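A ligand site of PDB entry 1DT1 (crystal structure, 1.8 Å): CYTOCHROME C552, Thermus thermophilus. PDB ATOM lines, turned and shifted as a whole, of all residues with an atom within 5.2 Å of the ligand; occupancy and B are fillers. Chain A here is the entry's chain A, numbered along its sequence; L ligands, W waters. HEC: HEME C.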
ATOM      1  N   ILE A   5      10.044 -13.658  -3.648  1.00  0.00           N
ATOM      2  CA  ILE A   5       9.828 -13.923  -2.229  1.00  0.00           C
ATOM      3  C   ILE A   5       9.862 -15.425  -1.987  1.00  0.00           C
ATOM      4  O   ILE A   5      10.381 -15.954  -0.998  1.00  0.00           O
ATOM      5  CB  ILE A   5       8.484 -13.339  -1.759  1.00  0.00           C
ATOM      6  CG1 ILE A   5       8.287 -11.860  -2.087  1.00  0.00           C
ATOM      7  CG2 ILE A   5       8.278 -13.564  -0.268  1.00  0.00           C
ATOM      8  CD1 ILE A   5       9.518 -11.017  -1.788  1.00  0.00           C
ATOM      9  N   TYR A   6       9.304 -16.175  -2.945  1.00  0.00           N
ATOM     10  CA  TYR A   6       9.180 -17.620  -2.714  1.00  0.00           C
ATOM     11  C   TYR A   6      10.528 -18.302  -2.535  1.00  0.00           C
ATOM     12  O   TYR A   6      10.645 -19.419  -2.000  1.00  0.00           O
ATOM     13  CB  TYR A   6       8.359 -18.243  -3.859  1.00  0.00           C
ATOM     14  CG  TYR A   6       8.131 -19.717  -3.598  1.00  0.00           C
ATOM     15  CD1 TYR A   6       7.203 -20.162  -2.672  1.00  0.00           C
ATOM     16  CD2 TYR A   6       8.888 -20.664  -4.287  1.00  0.00           C
ATOM     17  CE1 TYR A   6       7.037 -21.523  -2.455  1.00  0.00           C
ATOM     18  CE2 TYR A   6       8.716 -22.018  -4.070  1.00  0.00           C
ATOM     19  CZ  TYR A   6       7.781 -22.442  -3.148  1.00  0.00           C
ATOM     20  OH  TYR A   6       7.630 -23.790  -2.937  1.00  0.00           O
ATOM     21  N   GLN A   8      12.585 -17.677  -0.372  1.00  0.00           N
ATOM     22  CA  GLN A   8      12.669 -17.849   1.073  1.00  0.00           C
ATOM     23  C   GLN A   8      11.855 -19.054   1.539  1.00  0.00           C
ATOM     24  O   GLN A   8      11.915 -19.373   2.732  1.00  0.00           O
ATOM     25  CB  GLN A   8      12.159 -16.607   1.829  1.00  0.00           C
ATOM     26  CG  GLN A   8      12.982 -15.355   1.569  1.00  0.00           C
ATOM     27  CD  GLN A   8      12.445 -14.140   2.307  1.00  0.00           C
ATOM     28  OE1 GLN A   8      12.012 -14.199   3.455  1.00  0.00           O
ATOM     29  NE2 GLN A   8      12.467 -12.996   1.629  1.00  0.00           N
ATOM     30  N   CYS A   9      11.112 -19.673   0.630  1.00  0.00           N
ATOM     31  CA  CYS A   9      10.294 -20.833   0.959  1.00  0.00           C
ATOM     32  C   CYS A   9      10.786 -22.115   0.302  1.00  0.00           C
ATOM     33  O   CYS A   9      10.457 -23.219   0.741  1.00  0.00           O
ATOM     34  CB  CYS A   9       8.835 -20.658   0.494  1.00  0.00           C
ATOM     35  SG  CYS A   9       8.124 -19.039   0.793  1.00  0.00           S
ATOM     36  N   CYS A  12      12.481 -25.489   1.563  1.00  0.00           N
ATOM     37  CA  CYS A  12      11.654 -26.503   2.193  1.00  0.00           C
ATOM     38  C   CYS A  12      10.585 -27.005   1.251  1.00  0.00           C
ATOM     39  O   CYS A  12      10.567 -28.201   0.937  1.00  0.00           O
ATOM     40  CB  CYS A  12      11.010 -25.940   3.477  1.00  0.00           C
ATOM     41  SG  CYS A  12      12.281 -25.518   4.724  1.00  0.00           S
ATOM     42  N   HIS A  13       9.726 -26.094   0.786  1.00  0.00           N
ATOM     43  CA  HIS A  13       8.598 -26.495  -0.054  1.00  0.00           C
ATOM     44  C   HIS A  13       9.022 -26.766  -1.504  1.00  0.00           C
ATOM     45  O   HIS A  13       8.220 -27.281  -2.269  1.00  0.00           O
ATOM     46  CB  HIS A  13       7.482 -25.454   0.022  1.00  0.00           C
ATOM     47  CG  HIS A  13       6.896 -25.368   1.409  1.00  0.00           C
ATOM     48  ND1 HIS A  13       6.101 -26.342   1.969  1.00  0.00           N
ATOM     49  CD2 HIS A  13       6.996 -24.406   2.359  1.00  0.00           C
ATOM     50  CE1 HIS A  13       5.727 -26.009   3.191  1.00  0.00           C
ATOM     51  NE2 HIS A  13       6.270 -24.828   3.456  1.00  0.00           N
ATOM     52  N   ALA A  23       8.375 -34.483   5.265  1.00  0.00           N
ATOM     53  CA  ALA A  23       9.112 -33.387   5.901  1.00  0.00           C
ATOM     54  C   ALA A  23       8.428 -32.047   5.676  1.00  0.00           C
ATOM     55  O   ALA A  23       8.145 -31.325   6.626  1.00  0.00           O
ATOM     56  CB  ALA A  23      10.532 -33.308   5.366  1.00  0.00           C
ATOM     57  N   PHE A  24       8.210 -31.717   4.409  1.00  0.00           N
ATOM     58  CA  PHE A  24       7.701 -30.397   4.055  1.00  0.00           C
ATOM     59  C   PHE A  24       6.470 -30.567   3.177  1.00  0.00           C
ATOM     60  O   PHE A  24       6.618 -31.121   2.085  1.00  0.00           O
ATOM     61  CB  PHE A  24       8.786 -29.582   3.367  1.00  0.00           C
ATOM     62  CG  PHE A  24      10.096 -29.482   4.120  1.00  0.00           C
ATOM     63  CD1 PHE A  24      10.143 -28.979   5.405  1.00  0.00           C
ATOM     64  CD2 PHE A  24      11.298 -29.890   3.540  1.00  0.00           C
ATOM     65  CE1 PHE A  24      11.316 -28.874   6.123  1.00  0.00           C
ATOM     66  CE2 PHE A  24      12.483 -29.787   4.246  1.00  0.00           C
ATOM     67  CZ  PHE A  24      12.509 -29.277   5.533  1.00  0.00           C
ATOM     68  N   PRO A  25       5.291 -30.144   3.621  1.00  0.00           N
ATOM     69  CA  PRO A  25       4.091 -30.460   2.827  1.00  0.00           C
ATOM     70  C   PRO A  25       4.135 -29.816   1.451  1.00  0.00           C
ATOM     71  O   PRO A  25       4.671 -28.739   1.217  1.00  0.00           O
ATOM     72  CB  PRO A  25       2.932 -29.847   3.629  1.00  0.00           C
ATOM     73  CG  PRO A  25       3.522 -29.073   4.733  1.00  0.00           C
ATOM     74  CD  PRO A  25       4.979 -29.406   4.848  1.00  0.00           C
ATOM     75  N   LEU A  27       2.766 -27.613  -1.623  1.00  0.00           N
ATOM     76  CA  LEU A  27       1.914 -26.463  -1.877  1.00  0.00           C
ATOM     77  C   LEU A  27       1.195 -26.681  -3.205  1.00  0.00           C
ATOM     78  O   LEU A  27      -0.015 -26.498  -3.304  1.00  0.00           O
ATOM     79  CB  LEU A  27       2.699 -25.150  -1.880  1.00  0.00           C
ATOM     80  CG  LEU A  27       3.492 -24.863  -0.597  1.00  0.00           C
ATOM     81  CD1 LEU A  27       4.182 -23.506  -0.654  1.00  0.00           C
ATOM     82  CD2 LEU A  27       2.573 -24.938   0.620  1.00  0.00           C
ATOM     83  N   HIS A  30      -2.119 -28.449  -3.380  1.00  0.00           N
ATOM     84  CA  HIS A  30      -2.728 -28.499  -2.037  1.00  0.00           C
ATOM     85  C   HIS A  30      -3.274 -27.145  -1.631  1.00  0.00           C
ATOM     86  O   HIS A  30      -4.209 -27.010  -0.836  1.00  0.00           O
ATOM     87  CB  HIS A  30      -1.691 -29.033  -1.057  1.00  0.00           C
ATOM     88  CG  HIS A  30      -2.016 -28.958   0.402  1.00  0.00           C
ATOM     89  ND1 HIS A  30      -3.215 -29.394   0.920  1.00  0.00           N
ATOM     90  CD2 HIS A  30      -1.296 -28.505   1.456  1.00  0.00           C
ATOM     91  CE1 HIS A  30      -3.210 -29.205   2.233  1.00  0.00           C
ATOM     92  NE2 HIS A  30      -2.057 -28.669   2.588  1.00  0.00           N
ATOM     93  N   ILE A  34      -6.970 -25.952   0.350  1.00  0.00           N
ATOM     94  CA  ILE A  34      -7.136 -25.066   1.506  1.00  0.00           C
ATOM     95  C   ILE A  34      -8.087 -23.933   1.129  1.00  0.00           C
ATOM     96  O   ILE A  34      -9.001 -23.574   1.860  1.00  0.00           O
ATOM     97  CB  ILE A  34      -5.768 -24.540   1.963  1.00  0.00           C
ATOM     98  CG1 ILE A  34      -4.875 -25.632   2.574  1.00  0.00           C
ATOM     99  CG2 ILE A  34      -5.969 -23.354   2.899  1.00  0.00           C
ATOM    100  CD1 ILE A  34      -3.453 -25.216   2.869  1.00  0.00           C
ATOM    101  N   TYR A  43      -6.508 -18.550   6.621  1.00  0.00           N
ATOM    102  CA  TYR A  43      -5.593 -19.509   7.266  1.00  0.00           C
ATOM    103  C   TYR A  43      -4.216 -19.422   6.622  1.00  0.00           C
ATOM    104  O   TYR A  43      -3.203 -19.414   7.327  1.00  0.00           O
ATOM    105  CB  TYR A  43      -6.129 -20.947   7.215  1.00  0.00           C
ATOM    106  CG  TYR A  43      -5.074 -21.970   7.539  1.00  0.00           C
ATOM    107  CD1 TYR A  43      -4.643 -22.151   8.846  1.00  0.00           C
ATOM    108  CD2 TYR A  43      -4.493 -22.744   6.537  1.00  0.00           C
ATOM    109  CE1 TYR A  43      -3.670 -23.087   9.165  1.00  0.00           C
ATOM    110  CE2 TYR A  43      -3.516 -23.676   6.844  1.00  0.00           C
ATOM    111  CZ  TYR A  43      -3.120 -23.834   8.152  1.00  0.00           C
ATOM    112  OH  TYR A  43      -2.142 -24.768   8.427  1.00  0.00           O
ATOM    113  N   LEU A  44      -4.151 -19.350   5.298  1.00  0.00           N
ATOM    114  CA  LEU A  44      -2.853 -19.245   4.614  1.00  0.00           C
ATOM    115  C   LEU A  44      -2.079 -18.026   5.082  1.00  0.00           C
ATOM    116  O   LEU A  44      -0.852 -18.038   5.248  1.00  0.00           O
ATOM    117  CB  LEU A  44      -3.075 -19.181   3.091  1.00  0.00           C
ATOM    118  CG  LEU A  44      -3.564 -20.496   2.457  1.00  0.00           C
ATOM    119  CD1 LEU A  44      -3.925 -20.298   0.993  1.00  0.00           C
ATOM    120  CD2 LEU A  44      -2.524 -21.598   2.594  1.00  0.00           C
ATOM    121  N   VAL A  47      -0.620 -18.643   8.563  1.00  0.00           N
ATOM    122  CA  VAL A  47       0.567 -19.514   8.606  1.00  0.00           C
ATOM    123  C   VAL A  47       1.791 -18.637   8.399  1.00  0.00           C
ATOM    124  O   VAL A  47       2.795 -18.763   9.100  1.00  0.00           O
ATOM    125  CB  VAL A  47       0.539 -20.635   7.555  1.00  0.00           C
ATOM    126  CG1 VAL A  47       1.892 -21.329   7.440  1.00  0.00           C
ATOM    127  CG2 VAL A  47      -0.556 -21.646   7.863  1.00  0.00           C
ATOM    128  N   LEU A  48       1.647 -17.722   7.437  1.00  0.00           N
ATOM    129  CA  LEU A  48       2.818 -16.901   7.131  1.00  0.00           C
ATOM    130  C   LEU A  48       3.116 -15.880   8.222  1.00  0.00           C
ATOM    131  O   LEU A  48       4.282 -15.625   8.511  1.00  0.00           O
ATOM    132  CB  LEU A  48       2.628 -16.217   5.764  1.00  0.00           C
ATOM    133  CG  LEU A  48       3.306 -17.057   4.653  1.00  0.00           C
ATOM    134  CD1 LEU A  48       2.586 -18.386   4.487  1.00  0.00           C
ATOM    135  CD2 LEU A  48       3.371 -16.306   3.350  1.00  0.00           C
ATOM    136  N   LEU A  52       3.486 -22.414  12.136  1.00  0.00           N
ATOM    137  CA  LEU A  52       2.599 -23.554  12.264  1.00  0.00           C
ATOM    138  C   LEU A  52       3.350 -24.694  12.971  1.00  0.00           C
ATOM    139  O   LEU A  52       4.549 -24.846  12.800  1.00  0.00           O
ATOM    140  CB  LEU A  52       2.097 -24.011  10.898  1.00  0.00           C
ATOM    141  CG  LEU A  52       1.162 -25.221  10.844  1.00  0.00           C
ATOM    142  CD1 LEU A  52      -0.134 -24.988  11.618  1.00  0.00           C
ATOM    143  CD2 LEU A  52       0.838 -25.581   9.403  1.00  0.00           C
ATOM    144  N   GLN A  53       2.622 -25.466  13.770  1.00  0.00           N
ATOM    145  CA  GLN A  53       3.148 -26.672  14.386  1.00  0.00           C
ATOM    146  C   GLN A  53       2.053 -27.736  14.497  1.00  0.00           C
ATOM    147  O   GLN A  53       0.863 -27.483  14.302  1.00  0.00           O
ATOM    148  CB  GLN A  53       3.732 -26.385  15.779  1.00  0.00           C
ATOM    149  CG  GLN A  53       2.697 -26.028  16.833  1.00  0.00           C
ATOM    150  CD  GLN A  53       3.314 -25.454  18.089  1.00  0.00           C
ATOM    151  OE1 GLN A  53       4.265 -24.674  18.095  1.00  0.00           O
ATOM    152  NE2 GLN A  53       2.751 -25.845  19.226  1.00  0.00           N
ATOM    153  N   GLY A  54       2.459 -28.949  14.814  1.00  0.00           N
ATOM    154  CA  GLY A  54       1.485 -30.000  15.054  1.00  0.00           C
ATOM    155  C   GLY A  54       1.329 -30.997  13.945  1.00  0.00           C
ATOM    156  O   GLY A  54       1.748 -30.813  12.799  1.00  0.00           O
ATOM    157  N   GLN A  55       0.692 -32.122  14.299  1.00  0.00           N
ATOM    158  CA  GLN A  55       0.456 -33.161  13.305  1.00  0.00           C
ATOM    159  C   GLN A  55      -0.672 -32.739  12.373  1.00  0.00           C
ATOM    160  O   GLN A  55      -1.757 -32.340  12.782  1.00  0.00           O
ATOM    161  CB  GLN A  55       0.123 -34.477  13.991  1.00  0.00           C
ATOM    162  CG  GLN A  55      -0.197 -35.621  13.043  1.00  0.00           C
ATOM    163  CD  GLN A  55      -0.083 -36.967  13.734  1.00  0.00           C
ATOM    164  OE1 GLN A  55      -1.085 -37.646  13.945  1.00  0.00           O
ATOM    165  NE2 GLN A  55       1.139 -37.358  14.097  1.00  0.00           N
ATOM    166  N   ILE A  56      -0.379 -32.822  11.072  1.00  0.00           N
ATOM    167  CA  ILE A  56      -1.344 -32.499  10.046  1.00  0.00           C
ATOM    168  C   ILE A  56      -1.260 -33.582   8.971  1.00  0.00           C
ATOM    169  O   ILE A  56      -0.267 -34.323   8.980  1.00  0.00           O
ATOM    170  CB  ILE A  56      -1.105 -31.133   9.378  1.00  0.00           C
ATOM    171  CG1 ILE A  56       0.241 -31.052   8.657  1.00  0.00           C
ATOM    172  CG2 ILE A  56      -1.260 -30.009  10.383  1.00  0.00           C
ATOM    173  CD1 ILE A  56       0.446 -29.753   7.908  1.00  0.00           C
ATOM    174  N   VAL A  58      -1.599 -34.211   4.675  1.00  0.00           N
ATOM    175  CA  VAL A  58      -1.694 -33.572   3.363  1.00  0.00           C
ATOM    176  C   VAL A  58      -1.609 -34.656   2.288  1.00  0.00           C
ATOM    177  O   VAL A  58      -0.604 -35.360   2.242  1.00  0.00           O
ATOM    178  CB  VAL A  58      -0.612 -32.513   3.150  1.00  0.00           C
ATOM    179  CG1 VAL A  58      -0.675 -31.959   1.737  1.00  0.00           C
ATOM    180  CG2 VAL A  58      -0.740 -31.390   4.182  1.00  0.00           C
ATOM    181  N   TYR A  63       2.453 -35.112   8.367  1.00  0.00           N
ATOM    182  CA  TYR A  63       3.537 -34.201   8.669  1.00  0.00           C
ATOM    183  C   TYR A  63       3.470 -33.880  10.154  1.00  0.00           C
ATOM    184  O   TYR A  63       2.403 -33.852  10.763  1.00  0.00           O
ATOM    185  CB  TYR A  63       3.482 -32.919   7.823  1.00  0.00           C
ATOM    186  CG  TYR A  63       3.590 -33.312   6.348  1.00  0.00           C
ATOM    187  CD1 TYR A  63       2.463 -33.800   5.679  1.00  0.00           C
ATOM    188  CD2 TYR A  63       4.787 -33.205   5.665  1.00  0.00           C
ATOM    189  CE1 TYR A  63       2.550 -34.164   4.339  1.00  0.00           C
ATOM    190  CE2 TYR A  63       4.889 -33.568   4.331  1.00  0.00           C
ATOM    191  CZ  TYR A  63       3.768 -34.035   3.687  1.00  0.00           C
ATOM    192  OH  TYR A  63       3.850 -34.403   2.360  1.00  0.00           O
ATOM    193  N   ASN A  64       4.650 -33.664  10.735  1.00  0.00           N
ATOM    194  CA  ASN A  64       4.694 -33.404  12.180  1.00  0.00           C
ATOM    195  C   ASN A  64       5.859 -32.487  12.484  1.00  0.00           C
ATOM    196  O   ASN A  64       6.720 -32.796  13.317  1.00  0.00           O
ATOM    197  CB  ASN A  64       4.800 -34.727  12.930  1.00  0.00           C
ATOM    198  CG  ASN A  64       4.053 -34.688  14.248  1.00  0.00           C
ATOM    199  OD1 ASN A  64       3.274 -35.592  14.554  1.00  0.00           O
ATOM    200  ND2 ASN A  64       4.317 -33.609  14.983  1.00  0.00           N
ATOM    201  N   GLY A  65       5.895 -31.358  11.775  1.00  0.00           N
ATOM    202  CA  GLY A  65       7.031 -30.477  11.915  1.00  0.00           C
ATOM    203  C   GLY A  65       6.641 -29.106  12.441  1.00  0.00           C
ATOM    204  O   GLY A  65       5.599 -28.917  13.055  1.00  0.00           O
ATOM    205  N   VAL A  66       7.526 -28.154  12.184  1.00  0.00           N
ATOM    206  CA  VAL A  66       7.337 -26.789  12.636  1.00  0.00           C
ATOM    207  C   VAL A  66       7.708 -25.820  11.525  1.00  0.00           C
ATOM    208  O   VAL A  66       8.755 -25.937  10.881  1.00  0.00           O
ATOM    209  CB  VAL A  66       8.209 -26.499  13.879  1.00  0.00           C
ATOM    210  CG1 VAL A  66       8.125 -25.037  14.283  1.00  0.00           C
ATOM    211  CG2 VAL A  66       7.780 -27.396  15.037  1.00  0.00           C
ATOM    212  N   MET A  67       6.835 -24.839  11.321  1.00  0.00           N
ATOM    213  CA  MET A  67       7.184 -23.786  10.362  1.00  0.00           C
ATOM    214  C   MET A  67       7.317 -22.485  11.130  1.00  0.00           C
ATOM    215  O   MET A  67       6.454 -22.169  11.945  1.00  0.00           O
ATOM    216  CB  MET A  67       6.155 -23.625   9.245  1.00  0.00           C
ATOM    217  CG  MET A  67       6.462 -22.444   8.325  1.00  0.00           C
ATOM    218  SD  MET A  67       5.368 -22.417   6.898  1.00  0.00           S
ATOM    219  CE  MET A  67       5.388 -20.666   6.493  1.00  0.00           C
ATOM    220  N   PHE A  70       6.862 -15.750   9.318  1.00  0.00           N
ATOM    221  CA  PHE A  70       7.511 -14.883   8.353  1.00  0.00           C
ATOM    222  C   PHE A  70       6.998 -13.457   8.480  1.00  0.00           C
ATOM    223  O   PHE A  70       6.913 -12.750   7.475  1.00  0.00           O
ATOM    224  CB  PHE A  70       7.281 -15.401   6.923  1.00  0.00           C
ATOM    225  CG  PHE A  70       8.222 -16.569   6.591  1.00  0.00           C
ATOM    226  CD1 PHE A  70       7.963 -17.838   7.069  1.00  0.00           C
ATOM    227  CD2 PHE A  70       9.342 -16.375   5.795  1.00  0.00           C
ATOM    228  CE1 PHE A  70       8.806 -18.902   6.795  1.00  0.00           C
ATOM    229  CE2 PHE A  70      10.192 -17.433   5.518  1.00  0.00           C
ATOM    230  CZ  PHE A  70       9.931 -18.704   6.018  1.00  0.00           C
ATOM    231  N   LEU A  73       8.192 -10.271   6.832  1.00  0.00           N
ATOM    232  CA  LEU A  73       7.798  -9.821   5.489  1.00  0.00           C
ATOM    233  C   LEU A  73       6.722  -8.739   5.608  1.00  0.00           C
ATOM    234  O   LEU A  73       5.883  -8.810   6.510  1.00  0.00           O
ATOM    235  CB  LEU A  73       7.221 -10.955   4.657  1.00  0.00           C
ATOM    236  CG  LEU A  73       8.222 -12.067   4.287  1.00  0.00           C
ATOM    237  CD1 LEU A  73       7.480 -13.198   3.598  1.00  0.00           C
ATOM    238  CD2 LEU A  73       9.323 -11.482   3.423  1.00  0.00           C
ATOM    239  N   VAL A  81       3.692 -13.417  -2.152  1.00  0.00           N
ATOM    240  CA  VAL A  81       4.129 -14.827  -2.192  1.00  0.00           C
ATOM    241  C   VAL A  81       2.926 -15.759  -2.113  1.00  0.00           C
ATOM    242  O   VAL A  81       2.938 -16.870  -2.657  1.00  0.00           O
ATOM    243  CB  VAL A  81       5.147 -15.123  -1.090  1.00  0.00           C
ATOM    244  CG1 VAL A  81       4.512 -15.127   0.289  1.00  0.00           C
ATOM    245  CG2 VAL A  81       5.811 -16.481  -1.342  1.00  0.00           C
ATOM    246  N   LEU A  82       1.851 -15.351  -1.444  1.00  0.00           N
ATOM    247  CA  LEU A  82       0.668 -16.226  -1.427  1.00  0.00           C
ATOM    248  C   LEU A  82       0.040 -16.293  -2.815  1.00  0.00           C
ATOM    249  O   LEU A  82      -0.427 -17.340  -3.239  1.00  0.00           O
ATOM    250  CB  LEU A  82      -0.340 -15.719  -0.387  1.00  0.00           C
ATOM    251  CG  LEU A  82       0.084 -15.941   1.069  1.00  0.00           C
ATOM    252  CD1 LEU A  82      -0.902 -15.306   2.039  1.00  0.00           C
ATOM    253  CD2 LEU A  82       0.237 -17.439   1.327  1.00  0.00           C
ATOM    254  N   ILE A  85       2.188 -18.881  -4.645  1.00  0.00           N
ATOM    255  CA  ILE A  85       1.861 -20.283  -4.392  1.00  0.00           C
ATOM    256  C   ILE A  85       0.432 -20.589  -4.821  1.00  0.00           C
ATOM    257  O   ILE A  85       0.144 -21.762  -5.081  1.00  0.00           O
ATOM    258  CB  ILE A  85       2.106 -20.716  -2.935  1.00  0.00           C
ATOM    259  CG1 ILE A  85       1.117 -20.151  -1.925  1.00  0.00           C
ATOM    260  CG2 ILE A  85       3.552 -20.355  -2.546  1.00  0.00           C
ATOM    261  CD1 ILE A  85       1.285 -20.784  -0.535  1.00  0.00           C
ATOM    262  N   ARG A 123      -6.518 -24.274  11.483  1.00  0.00           N
ATOM    263  CA  ARG A 123      -6.500 -25.255  10.407  1.00  0.00           C
ATOM    264  C   ARG A 123      -7.572 -26.305  10.625  1.00  0.00           C
ATOM    265  O   ARG A 123      -8.319 -26.718   9.747  1.00  0.00           O
ATOM    266  CB  ARG A 123      -5.125 -25.913  10.320  1.00  0.00           C
ATOM    267  CG  ARG A 123      -4.940 -26.773   9.068  1.00  0.00           C
ATOM    268  CD  ARG A 123      -3.654 -27.574   9.187  1.00  0.00           C
ATOM    269  NE  ARG A 123      -3.293 -28.212   7.923  1.00  0.00           N
ATOM    270  CZ  ARG A 123      -3.670 -29.408   7.519  1.00  0.00           C
ATOM    271  NH1 ARG A 123      -4.451 -30.179   8.266  1.00  0.00           N
ATOM    272  NH2 ARG A 123      -3.267 -29.863   6.334  1.00  0.00           N
HETATM  273 FE   HEC L   1       5.997 -23.673   5.072  1.00  0.00          FE
HETATM  274  CHA HEC L   1       3.493 -25.498   6.425  1.00  0.00           C
HETATM  275  CHB HEC L   1       3.872 -22.076   3.066  1.00  0.00           C
HETATM  276  CHC HEC L   1       8.436 -21.419   4.370  1.00  0.00           C
HETATM  277  CHD HEC L   1       8.283 -25.669   6.599  1.00  0.00           C
HETATM  278  NA  HEC L   1       3.956 -23.723   4.827  1.00  0.00           N
HETATM  279  C1A HEC L   1       3.090 -24.526   5.453  1.00  0.00           C
HETATM  280  C2A HEC L   1       1.804 -24.239   5.026  1.00  0.00           C
HETATM  281  C3A HEC L   1       1.917 -23.217   4.085  1.00  0.00           C
HETATM  282  C4A HEC L   1       3.265 -22.933   4.019  1.00  0.00           C
HETATM  283  CMA HEC L   1       0.847 -22.556   3.225  1.00  0.00           C
HETATM  284  CAA HEC L   1       0.528 -24.915   5.518  1.00  0.00           C
HETATM  285  CBA HEC L   1       0.099 -26.152   4.767  1.00  0.00           C
HETATM  286  CGA HEC L   1      -1.082 -26.895   5.425  1.00  0.00           C
HETATM  287  O1A HEC L   1      -1.528 -27.914   4.915  1.00  0.00           O
HETATM  288  O2A HEC L   1      -1.575 -26.465   6.456  1.00  0.00           O
HETATM  289  NB  HEC L   1       6.129 -21.981   3.928  1.00  0.00           N
HETATM  290  C1B HEC L   1       5.149 -21.491   3.168  1.00  0.00           C
HETATM  291  C2B HEC L   1       5.572 -20.337   2.504  1.00  0.00           C
HETATM  292  C3B HEC L   1       6.873 -20.126   2.934  1.00  0.00           C
HETATM  293  C4B HEC L   1       7.187 -21.176   3.777  1.00  0.00           C
HETATM  294  CMB HEC L   1       4.705 -19.602   1.486  1.00  0.00           C
HETATM  295  CAB HEC L   1       7.719 -19.065   2.561  1.00  0.00           C
HETATM  296  CBB HEC L   1       7.195 -17.697   2.579  1.00  0.00           C
HETATM  297  NC  HEC L   1       8.031 -23.582   5.445  1.00  0.00           N
HETATM  298  C1C HEC L   1       8.849 -22.621   4.999  1.00  0.00           C
HETATM  299  C2C HEC L   1      10.196 -22.929   5.239  1.00  0.00           C
HETATM  300  C3C HEC L   1      10.172 -24.204   5.836  1.00  0.00           C
HETATM  301  C4C HEC L   1       8.834 -24.544   5.967  1.00  0.00           C
HETATM  302  CMC HEC L   1      11.381 -21.998   4.932  1.00  0.00           C
HETATM  303  CAC HEC L   1      11.299 -24.977   6.194  1.00  0.00           C
HETATM  304  CBC HEC L   1      12.312 -24.485   7.151  1.00  0.00           C
HETATM  305  ND  HEC L   1       5.915 -25.312   6.339  1.00  0.00           N
HETATM  306  C1D HEC L   1       6.952 -25.997   6.831  1.00  0.00           C
HETATM  307  C2D HEC L   1       6.523 -27.098   7.556  1.00  0.00           C
HETATM  308  C3D HEC L   1       5.123 -27.021   7.548  1.00  0.00           C
HETATM  309  C4D HEC L   1       4.788 -25.934   6.731  1.00  0.00           C
HETATM  310  CMD HEC L   1       7.349 -28.137   8.284  1.00  0.00           C
HETATM  311  CAD HEC L   1       4.216 -27.995   8.303  1.00  0.00           C
HETATM  312  CBD HEC L   1       4.240 -27.777   9.837  1.00  0.00           C
HETATM  313  CGD HEC L   1       3.530 -28.894  10.607  1.00  0.00           C
HETATM  314  O1D HEC L   1       2.694 -28.606  11.456  1.00  0.00           O
HETATM  315  O2D HEC L   1       3.817 -30.044  10.330  1.00  0.00           O
HETATM  316  O   HOH W   1      10.157 -22.286   8.811  1.00  0.00           O
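The side-chain sulfur (SG) of Cys 9 is covalently linked to a carbon (CAB) of the ligand (1.8 Å). The side-chain sulfur (SG) of Cys 12 is covalently linked to a carbon (CAC) of the ligand, at 1.8 Å. FE of the ligand is bound by NE2 of His 13 (2.0 Å). FE of the ligand is bound by SD of Met 67. A ring nitrogen (NE2) of His 30 lies within hydrogen-bond range of an oxygen (O1A) of the ligand, 2.5 Å away. OH of Tyr 43 is in hydrogen-bond range of O2A of the ligand (2.7 Å). An oxygen (O1D) of the ligand is in hydrogen-bond range of the backbone NH (N) of Gly 54 (3.4 Å). O of Gly 54 lies close to O1D of the ligand, at 2.8 Å. N of Gly 65 is in hydrogen-bond range of O2D of the ligand, at 2.9 Å. O2A of the ligand is in salt-bridge range of NE of Arg 123.
O of Pro 25 sits at hydrogen-bond distance from ND1 of His 13 (2.9 Å). The backbone NH (N) of Met 67 lies within hydrogen-bond range of the backbone carbonyl oxygen (O) of Leu 52, 2.7 Å away. N of Phe 70 sits at hydrogen-bond distance from O of Leu 48, 2.7 Å away. The side-chain amide nitrogen (NE2) of Gln 55 sits at hydrogen-bond distance from the side-chain amide oxygen (OD1) of Asn 64 (2.8 Å). N of Tyr 63 is in hydrogen-bond range of O of Ile 56, 2.9 Å away.
O of Gln 8 touches CMC of the ligand (3.5 Å). Ala 23 touches the ligand (O to CMD, 3.7 Å). Phe 24 touches the ligand (CE1 to CAC, 3.9 Å). Pro 25 touches the ligand (CD to C3D, 3.6 Å). Leu 27 touches the ligand (CD2 to C3A, 3.9 Å). CD1 of Ile 34 touches CGA of the ligand, at 3.9 Å. Leu 44 touches the ligand (CD2 to CMA, 3.6 Å). CG1 of Val 47 touches C2A of the ligand, 3.8 Å away. CD1 of Leu 48 touches CMB of the ligand, at 3.9 Å. Leu 52 touches the ligand (CG to O1D, 3.8 Å). Gln 53 touches the ligand (C to O1D, 3.2 Å). Val 58 touches the ligand (CG2 to O1A, 3.6 Å). Tyr 63 touches the ligand (CB to O2D, 3.8 Å). Asn 64 touches the ligand (N to O2D, 3.7 Å). Val 66 touches the ligand. Phe 70 touches the ligand. Hydrophobic or aromatic side chains that line the ligand: His 13, Phe 24, Pro 25, Leu 27, His 30, Ile 34, Tyr 43, Leu 44, Val 47, Leu 48, Leu 52, Val 58, Tyr 63, Met 67 and Phe 70. 25 residues have an atom within 4 Å of the ligand: Gln 8, Cys 9, Cys 12, His 13, Ala 23, Phe 24, Pro 25, Leu 27, His 30, Ile 34, Tyr 43, Leu 44, Val 47, Leu 48, Leu 52, Gln 53, Gly 54, Val 58, Tyr 63, Asn 64, Gly 65, Val 66, Met 67, Phe 70 and Arg 123. The nearest printed residue that does not touch the ligand is Ile 56 (4.03 Å).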
